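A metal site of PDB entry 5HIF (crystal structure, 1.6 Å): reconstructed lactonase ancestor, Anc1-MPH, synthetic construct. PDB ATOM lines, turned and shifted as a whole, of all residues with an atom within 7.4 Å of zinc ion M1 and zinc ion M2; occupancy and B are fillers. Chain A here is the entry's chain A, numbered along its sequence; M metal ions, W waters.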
ATOM      1  N   SER A  68     -19.739   1.642  21.954  1.00  0.00           N
ATOM      2  CA  SER A  68     -18.429   2.054  22.435  1.00  0.00           C
ATOM      3  C   SER A  68     -17.577   2.665  21.323  1.00  0.00           C
ATOM      4  O   SER A  68     -17.697   2.315  20.181  1.00  0.00           O
ATOM      5  CB  SER A  68     -17.720   0.913  22.998  1.00  0.00           C
ATOM      6  OG  SER A  68     -18.292   0.522  24.263  1.00  0.00           O
ATOM      7  N   VAL A  69     -16.716   3.557  21.770  1.00  0.00           N
ATOM      8  CA  VAL A  69     -15.670   4.168  20.976  1.00  0.00           C
ATOM      9  C   VAL A  69     -14.377   3.984  21.700  1.00  0.00           C
ATOM     10  O   VAL A  69     -14.142   4.633  22.725  1.00  0.00           O
ATOM     11  CB  VAL A  69     -15.909   5.626  20.660  1.00  0.00           C
ATOM     12  CG1 VAL A  69     -14.728   6.241  19.790  1.00  0.00           C
ATOM     13  CG2 VAL A  69     -17.224   5.864  19.908  1.00  0.00           C
ATOM     14  N   ASN A  70     -13.522   3.140  21.168  1.00  0.00           N
ATOM     15  CA  ASN A  70     -12.258   2.699  21.868  1.00  0.00           C
ATOM     16  C   ASN A  70     -11.030   3.131  21.132  1.00  0.00           C
ATOM     17  O   ASN A  70     -11.021   3.213  19.886  1.00  0.00           O
ATOM     18  CB  ASN A  70     -12.242   1.214  22.020  1.00  0.00           C
ATOM     19  CG  ASN A  70     -13.533   0.576  22.573  1.00  0.00           C
ATOM     20  OD1 ASN A  70     -14.192   1.171  23.457  1.00  0.00           O
ATOM     21  ND2 ASN A  70     -13.892  -0.609  22.091  1.00  0.00           N
ATOM     22  N   ASP A  84      -5.553   5.222  17.587  1.00  0.00           N
ATOM     23  CA  ASP A  84      -6.751   6.050  17.604  1.00  0.00           C
ATOM     24  C   ASP A  84      -6.879   6.951  18.844  1.00  0.00           C
ATOM     25  O   ASP A  84      -6.113   6.827  19.793  1.00  0.00           O
ATOM     26  CB  ASP A  84      -7.978   5.258  17.352  1.00  0.00           C
ATOM     27  CG  ASP A  84      -8.033   4.679  15.932  1.00  0.00           C
ATOM     28  OD1 ASP A  84      -7.313   5.214  15.058  1.00  0.00           O
ATOM     29  OD2 ASP A  84      -8.843   3.751  15.689  1.00  0.00           O
ATOM     30  N   THR A 118      -6.359   4.378  12.571  1.00  0.00           N
ATOM     31  CA  THR A 118      -6.898   3.340  11.722  1.00  0.00           C
ATOM     32  C   THR A 118      -7.575   3.944  10.434  1.00  0.00           C
ATOM     33  O   THR A 118      -7.376   3.451   9.356  1.00  0.00           O
ATOM     34  CB  THR A 118      -7.918   2.421  12.479  1.00  0.00           C
ATOM     35  OG1 THR A 118      -8.999   3.248  12.965  1.00  0.00           O
ATOM     36  CG2 THR A 118      -7.223   1.651  13.585  1.00  0.00           C
ATOM     37  N   HIS A 119      -8.239   5.056  10.670  1.00  0.00           N
ATOM     38  CA  HIS A 119      -8.865   5.816   9.583  1.00  0.00           C
ATOM     39  C   HIS A 119      -9.330   7.141  10.082  1.00  0.00           C
ATOM     40  O   HIS A 119      -9.510   7.339  11.286  1.00  0.00           O
ATOM     41  CB  HIS A 119     -10.044   5.017   9.007  1.00  0.00           C
ATOM     42  CG  HIS A 119     -11.203   4.816   9.945  1.00  0.00           C
ATOM     43  ND1 HIS A 119     -11.093   4.132  11.157  1.00  0.00           N
ATOM     44  CD2 HIS A 119     -12.506   5.149   9.809  1.00  0.00           C
ATOM     45  CE1 HIS A 119     -12.275   4.082  11.732  1.00  0.00           C
ATOM     46  NE2 HIS A 119     -13.173   4.646  10.929  1.00  0.00           N
ATOM     47  N   MET A 120      -9.519   8.086   9.173  1.00  0.00           N
ATOM     48  CA  MET A 120      -9.782   9.464   9.600  1.00  0.00           C
ATOM     49  C   MET A 120     -11.245   9.871   9.816  1.00  0.00           C
ATOM     50  O   MET A 120     -11.592  11.029   9.625  1.00  0.00           O
ATOM     51  CB  MET A 120      -9.081  10.461   8.641  1.00  0.00           C
ATOM     52  CG  MET A 120      -7.570  10.233   8.680  1.00  0.00           C
ATOM     53  SD  MET A 120      -6.725  11.480   7.642  1.00  0.00           S
ATOM     54  CE  MET A 120      -5.060  10.872   7.820  1.00  0.00           C
ATOM     55  N   HIS A 121     -12.063   8.968  10.289  1.00  0.00           N
ATOM     56  CA  HIS A 121     -13.338   9.346  10.789  1.00  0.00           C
ATOM     57  C   HIS A 121     -13.222  10.126  12.070  1.00  0.00           C
ATOM     58  O   HIS A 121     -12.229  10.044  12.809  1.00  0.00           O
ATOM     59  CB  HIS A 121     -14.211   8.092  10.954  1.00  0.00           C
ATOM     60  CG  HIS A 121     -14.801   7.563   9.678  1.00  0.00           C
ATOM     61  ND1 HIS A 121     -15.412   6.339   9.542  1.00  0.00           N
ATOM     62  CD2 HIS A 121     -14.858   8.140   8.431  1.00  0.00           C
ATOM     63  CE1 HIS A 121     -15.839   6.158   8.294  1.00  0.00           C
ATOM     64  NE2 HIS A 121     -15.513   7.247   7.633  1.00  0.00           N
ATOM     65  N   PRO A 122     -14.229  10.958  12.368  1.00  0.00           N
ATOM     66  CA  PRO A 122     -14.106  11.933  13.474  1.00  0.00           C
ATOM     67  C   PRO A 122     -13.877  11.309  14.829  1.00  0.00           C
ATOM     68  O   PRO A 122     -13.199  11.911  15.625  1.00  0.00           O
ATOM     69  CB  PRO A 122     -15.445  12.655  13.474  1.00  0.00           C
ATOM     70  CG  PRO A 122     -16.315  11.794  12.726  1.00  0.00           C
ATOM     71  CD  PRO A 122     -15.500  11.143  11.639  1.00  0.00           C
ATOM     72  N   ASP A 123     -14.446  10.161  15.022  1.00  0.00           N
ATOM     73  CA  ASP A 123     -14.343   9.397  16.249  1.00  0.00           C
ATOM     74  C   ASP A 123     -13.046   8.664  16.393  1.00  0.00           C
ATOM     75  O   ASP A 123     -12.857   8.002  17.431  1.00  0.00           O
ATOM     76  CB  ASP A 123     -15.537   8.461  16.425  1.00  0.00           C
ATOM     77  CG  ASP A 123     -15.734   7.461  15.248  1.00  0.00           C
ATOM     78  OD1 ASP A 123     -15.671   7.922  14.099  1.00  0.00           O
ATOM     79  OD2 ASP A 123     -15.894   6.259  15.519  1.00  0.00           O
ATOM     80  N   HIS A 124     -12.125   8.855  15.478  1.00  0.00           N
ATOM     81  CA  HIS A 124     -10.746   8.337  15.583  1.00  0.00           C
ATOM     82  C   HIS A 124      -9.685   9.360  15.615  1.00  0.00           C
ATOM     83  O   HIS A 124      -8.614   9.145  16.243  1.00  0.00           O
ATOM     84  CB  HIS A 124     -10.492   7.295  14.507  1.00  0.00           C
ATOM     85  CG  HIS A 124     -11.529   6.182  14.542  1.00  0.00           C
ATOM     86  ND1 HIS A 124     -11.325   4.950  15.108  1.00  0.00           N
ATOM     87  CD2 HIS A 124     -12.842   6.212  14.191  1.00  0.00           C
ATOM     88  CE1 HIS A 124     -12.435   4.243  15.068  1.00  0.00           C
ATOM     89  NE2 HIS A 124     -13.400   5.021  14.552  1.00  0.00           N
ATOM     90  N   PHE A 167     -17.145  15.353   8.133  1.00  0.00           N
ATOM     91  CA  PHE A 167     -16.109  14.372   8.306  1.00  0.00           C
ATOM     92  C   PHE A 167     -14.789  14.940   7.768  1.00  0.00           C
ATOM     93  O   PHE A 167     -13.702  14.729   8.384  1.00  0.00           O
ATOM     94  CB  PHE A 167     -16.375  13.031   7.608  1.00  0.00           C
ATOM     95  CG  PHE A 167     -17.495  12.238   8.212  1.00  0.00           C
ATOM     96  CD1 PHE A 167     -18.334  12.758   9.223  1.00  0.00           C
ATOM     97  CD2 PHE A 167     -17.739  10.949   7.711  1.00  0.00           C
ATOM     98  CE1 PHE A 167     -19.374  11.987   9.737  1.00  0.00           C
ATOM     99  CE2 PHE A 167     -18.773  10.175   8.232  1.00  0.00           C
ATOM    100  CZ  PHE A 167     -19.596  10.699   9.231  1.00  0.00           C
ATOM    101  N   HIS A 205     -13.678   0.229   4.557  1.00  0.00           N
ATOM    102  CA  HIS A 205     -14.419   1.135   5.391  1.00  0.00           C
ATOM    103  C   HIS A 205     -14.117   2.606   5.078  1.00  0.00           C
ATOM    104  O   HIS A 205     -14.967   3.479   5.059  1.00  0.00           O
ATOM    105  CB  HIS A 205     -14.136   0.835   6.874  1.00  0.00           C
ATOM    106  CG  HIS A 205     -14.859   1.736   7.830  1.00  0.00           C
ATOM    107  ND1 HIS A 205     -16.260   1.781   7.954  1.00  0.00           N
ATOM    108  CD2 HIS A 205     -14.379   2.653   8.694  1.00  0.00           C
ATOM    109  CE1 HIS A 205     -16.569   2.722   8.825  1.00  0.00           C
ATOM    110  NE2 HIS A 205     -15.446   3.219   9.326  1.00  0.00           N
ATOM    111  N   THR A 206     -12.845   2.884   4.881  1.00  0.00           N
ATOM    112  CA  THR A 206     -12.325   4.101   4.229  1.00  0.00           C
ATOM    113  C   THR A 206     -11.226   3.654   3.228  1.00  0.00           C
ATOM    114  O   THR A 206     -10.681   2.595   3.341  1.00  0.00           O
ATOM    115  CB  THR A 206     -11.824   5.106   5.251  1.00  0.00           C
ATOM    116  OG1 THR A 206     -10.580   4.614   5.807  1.00  0.00           O
ATOM    117  CG2 THR A 206     -12.867   5.471   6.295  1.00  0.00           C
ATOM    118  N   HIS A 209      -8.207   2.572   5.297  1.00  0.00           N
ATOM    119  CA  HIS A 209      -8.419   1.957   6.584  1.00  0.00           C
ATOM    120  C   HIS A 209      -7.301   0.928   6.846  1.00  0.00           C
ATOM    121  O   HIS A 209      -6.991   0.117   5.971  1.00  0.00           O
ATOM    122  CB  HIS A 209      -9.818   1.318   6.645  1.00  0.00           C
ATOM    123  CG  HIS A 209     -10.125   0.780   8.019  1.00  0.00           C
ATOM    124  ND1 HIS A 209      -9.630  -0.421   8.453  1.00  0.00           N
ATOM    125  CD2 HIS A 209     -10.815   1.302   9.040  1.00  0.00           C
ATOM    126  CE1 HIS A 209      -9.996  -0.596   9.723  1.00  0.00           C
ATOM    127  NE2 HIS A 209     -10.749   0.404  10.090  1.00  0.00           N
ATOM    128  N   GLY A 225      -9.641  -1.497  14.133  1.00  0.00           N
ATOM    129  CA  GLY A 225     -10.344  -0.248  13.763  1.00  0.00           C
ATOM    130  C   GLY A 225     -11.843  -0.465  13.655  1.00  0.00           C
ATOM    131  O   GLY A 225     -12.459  -0.987  14.568  1.00  0.00           O
ATOM    132  N   ASP A 226     -12.348  -0.098  12.493  1.00  0.00           N
ATOM    133  CA  ASP A 226     -13.782  -0.215  12.201  1.00  0.00           C
ATOM    134  C   ASP A 226     -14.129  -1.313  11.214  1.00  0.00           C
ATOM    135  O   ASP A 226     -15.060  -1.159  10.396  1.00  0.00           O
ATOM    136  CB  ASP A 226     -14.332   1.153  11.703  1.00  0.00           C
ATOM    137  CG  ASP A 226     -14.529   2.156  12.823  1.00  0.00           C
ATOM    138  OD1 ASP A 226     -14.004   1.923  13.940  1.00  0.00           O
ATOM    139  OD2 ASP A 226     -15.168   3.223  12.559  1.00  0.00           O
ATOM    140  N   ILE A 228     -15.739  -3.713  12.225  1.00  0.00           N
ATOM    141  CA  ILE A 228     -17.064  -4.125  12.777  1.00  0.00           C
ATOM    142  C   ILE A 228     -17.685  -2.942  13.493  1.00  0.00           C
ATOM    143  O   ILE A 228     -16.986  -2.112  14.059  1.00  0.00           O
ATOM    144  CB  ILE A 228     -16.919  -5.391  13.604  1.00  0.00           C
ATOM    145  CG1 ILE A 228     -18.266  -5.887  14.098  1.00  0.00           C
ATOM    146  CG2 ILE A 228     -16.007  -5.143  14.717  1.00  0.00           C
ATOM    147  CD1 ILE A 228     -18.349  -7.351  14.430  1.00  0.00           C
ATOM    148  N   HIS A 229     -19.010  -2.786  13.401  1.00  0.00           N
ATOM    149  CA  HIS A 229     -19.760  -1.826  14.125  1.00  0.00           C
ATOM    150  C   HIS A 229     -20.802  -2.377  15.095  1.00  0.00           C
ATOM    151  O   HIS A 229     -21.089  -1.707  16.086  1.00  0.00           O
ATOM    152  CB  HIS A 229     -20.471  -0.796  13.238  1.00  0.00           C
ATOM    153  CG  HIS A 229     -19.524   0.108  12.498  1.00  0.00           C
ATOM    154  ND1 HIS A 229     -18.767  -0.322  11.429  1.00  0.00           N
ATOM    155  CD2 HIS A 229     -19.199   1.400  12.705  1.00  0.00           C
ATOM    156  CE1 HIS A 229     -18.031   0.675  10.998  1.00  0.00           C
ATOM    157  NE2 HIS A 229     -18.299   1.733  11.728  1.00  0.00           N
ATOM    158  N   PHE A 244     -21.707   3.845   6.952  1.00  0.00           N
ATOM    159  CA  PHE A 244     -20.459   4.537   7.214  1.00  0.00           C
ATOM    160  C   PHE A 244     -19.282   4.023   6.325  1.00  0.00           C
ATOM    161  O   PHE A 244     -18.247   4.659   6.277  1.00  0.00           O
ATOM    162  CB  PHE A 244     -20.053   4.357   8.680  1.00  0.00           C
ATOM    163  CG  PHE A 244     -21.018   4.895   9.684  1.00  0.00           C
ATOM    164  CD1 PHE A 244     -21.675   6.096   9.491  1.00  0.00           C
ATOM    165  CD2 PHE A 244     -21.263   4.174  10.859  1.00  0.00           C
ATOM    166  CE1 PHE A 244     -22.545   6.598  10.439  1.00  0.00           C
ATOM    167  CE2 PHE A 244     -22.132   4.681  11.794  1.00  0.00           C
ATOM    168  CZ  PHE A 244     -22.729   5.926  11.593  1.00  0.00           C
ATOM    169  N   ASP A 245     -19.373   2.857   5.713  1.00  0.00           N
ATOM    170  CA  ASP A 245     -18.353   2.352   4.841  1.00  0.00           C
ATOM    171  C   ASP A 245     -18.229   3.147   3.568  1.00  0.00           C
ATOM    172  O   ASP A 245     -19.238   3.378   2.892  1.00  0.00           O
ATOM    173  CB  ASP A 245     -18.586   0.899   4.431  1.00  0.00           C
ATOM    174  CG  ASP A 245     -18.594  -0.074   5.627  1.00  0.00           C
ATOM    175  OD1 ASP A 245     -17.746   0.061   6.568  1.00  0.00           O
ATOM    176  OD2 ASP A 245     -19.359  -1.069   5.553  1.00  0.00           O
ATOM    177  N   ALA A 272     -12.578  -0.880  17.706  1.00  0.00           N
ATOM    178  CA  ALA A 272     -13.039   0.442  18.158  1.00  0.00           C
ATOM    179  C   ALA A 272     -14.479   0.509  18.590  1.00  0.00           C
ATOM    180  O   ALA A 272     -14.785   1.316  19.502  1.00  0.00           O
ATOM    181  CB  ALA A 272     -12.826   1.487  17.035  1.00  0.00           C
ATOM    182  N   HIS A 273     -15.316  -0.371  18.027  1.00  0.00           N
ATOM    183  CA  HIS A 273     -16.769  -0.294  18.294  1.00  0.00           C
ATOM    184  C   HIS A 273     -17.352  -1.589  18.872  1.00  0.00           C
ATOM    185  O   HIS A 273     -18.579  -1.757  18.864  1.00  0.00           O
ATOM    186  CB  HIS A 273     -17.584   0.232  17.052  1.00  0.00           C
ATOM    187  CG  HIS A 273     -17.107   1.587  16.607  1.00  0.00           C
ATOM    188  ND1 HIS A 273     -16.985   2.654  17.445  1.00  0.00           N
ATOM    189  CD2 HIS A 273     -16.710   2.000  15.409  1.00  0.00           C
ATOM    190  CE1 HIS A 273     -16.531   3.712  16.770  1.00  0.00           C
ATOM    191  NE2 HIS A 273     -16.327   3.326  15.551  1.00  0.00           N
HETATM  192 ZN    ZN M   1     -15.411   4.620  14.219  1.00  0.00          ZN
HETATM  193 ZN    ZN M   2     -15.357   4.703  10.979  1.00  0.00          ZN
HETATM  194  O   HOH W   1     -15.846   5.666  12.592  1.00  0.00           O
HETATM  195  O   HOH W   2     -17.631   4.399  10.974  1.00  0.00           O
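The nearest printed residue that does not touch zinc ion M2 is His 124 (4.1 Å).
Zinc ion M1 is bound by water W1, NE2 of His 273, NE2 of His 124, OD2 of Asp 123 and OD2 of Asp 226.
ND1 of His 273 lies within hydrogen-bond range of O of Ser 68 (2.8 Å).
A ring nitrogen (ND1) of His 124 lies within hydrogen-bond range of the side-chain carboxylate (OD2) of Asp 84 (2.8 Å).
A ring nitrogen (NE2) of His 209 is in hydrogen-bond range of the backbone NH (N) of Asp 226, 2.9 Å away.
ND1 of His 119 lies within hydrogen-bond range of OG1 of Thr 118, at 2.9 Å.
The side-chain carboxylate (OD1) of Asp 245 is in hydrogen-bond range of a ring nitrogen (ND1) of His 205 (2.7 Å).
Zinc ion M2 is bound by water W1 (1.9 Å), the side-chain carboxylate of Asp 226 (2.2 Å), a ring nitrogen (ND1) of His 121 (2.2 Å), a ring nitrogen (NE2) of His 119 (2.2 Å), a ring nitrogen (NE2) of His 205 (2.2 Å) and water W2 (2.3 Å).
Zinc ion M2 has six donor atoms within binding distance.
Of the 23 residues printed, 5 come within 4 Å of zinc ion M1.
The nearest printed residue that does not touch zinc ion M1 is His 229 (4.8 Å).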
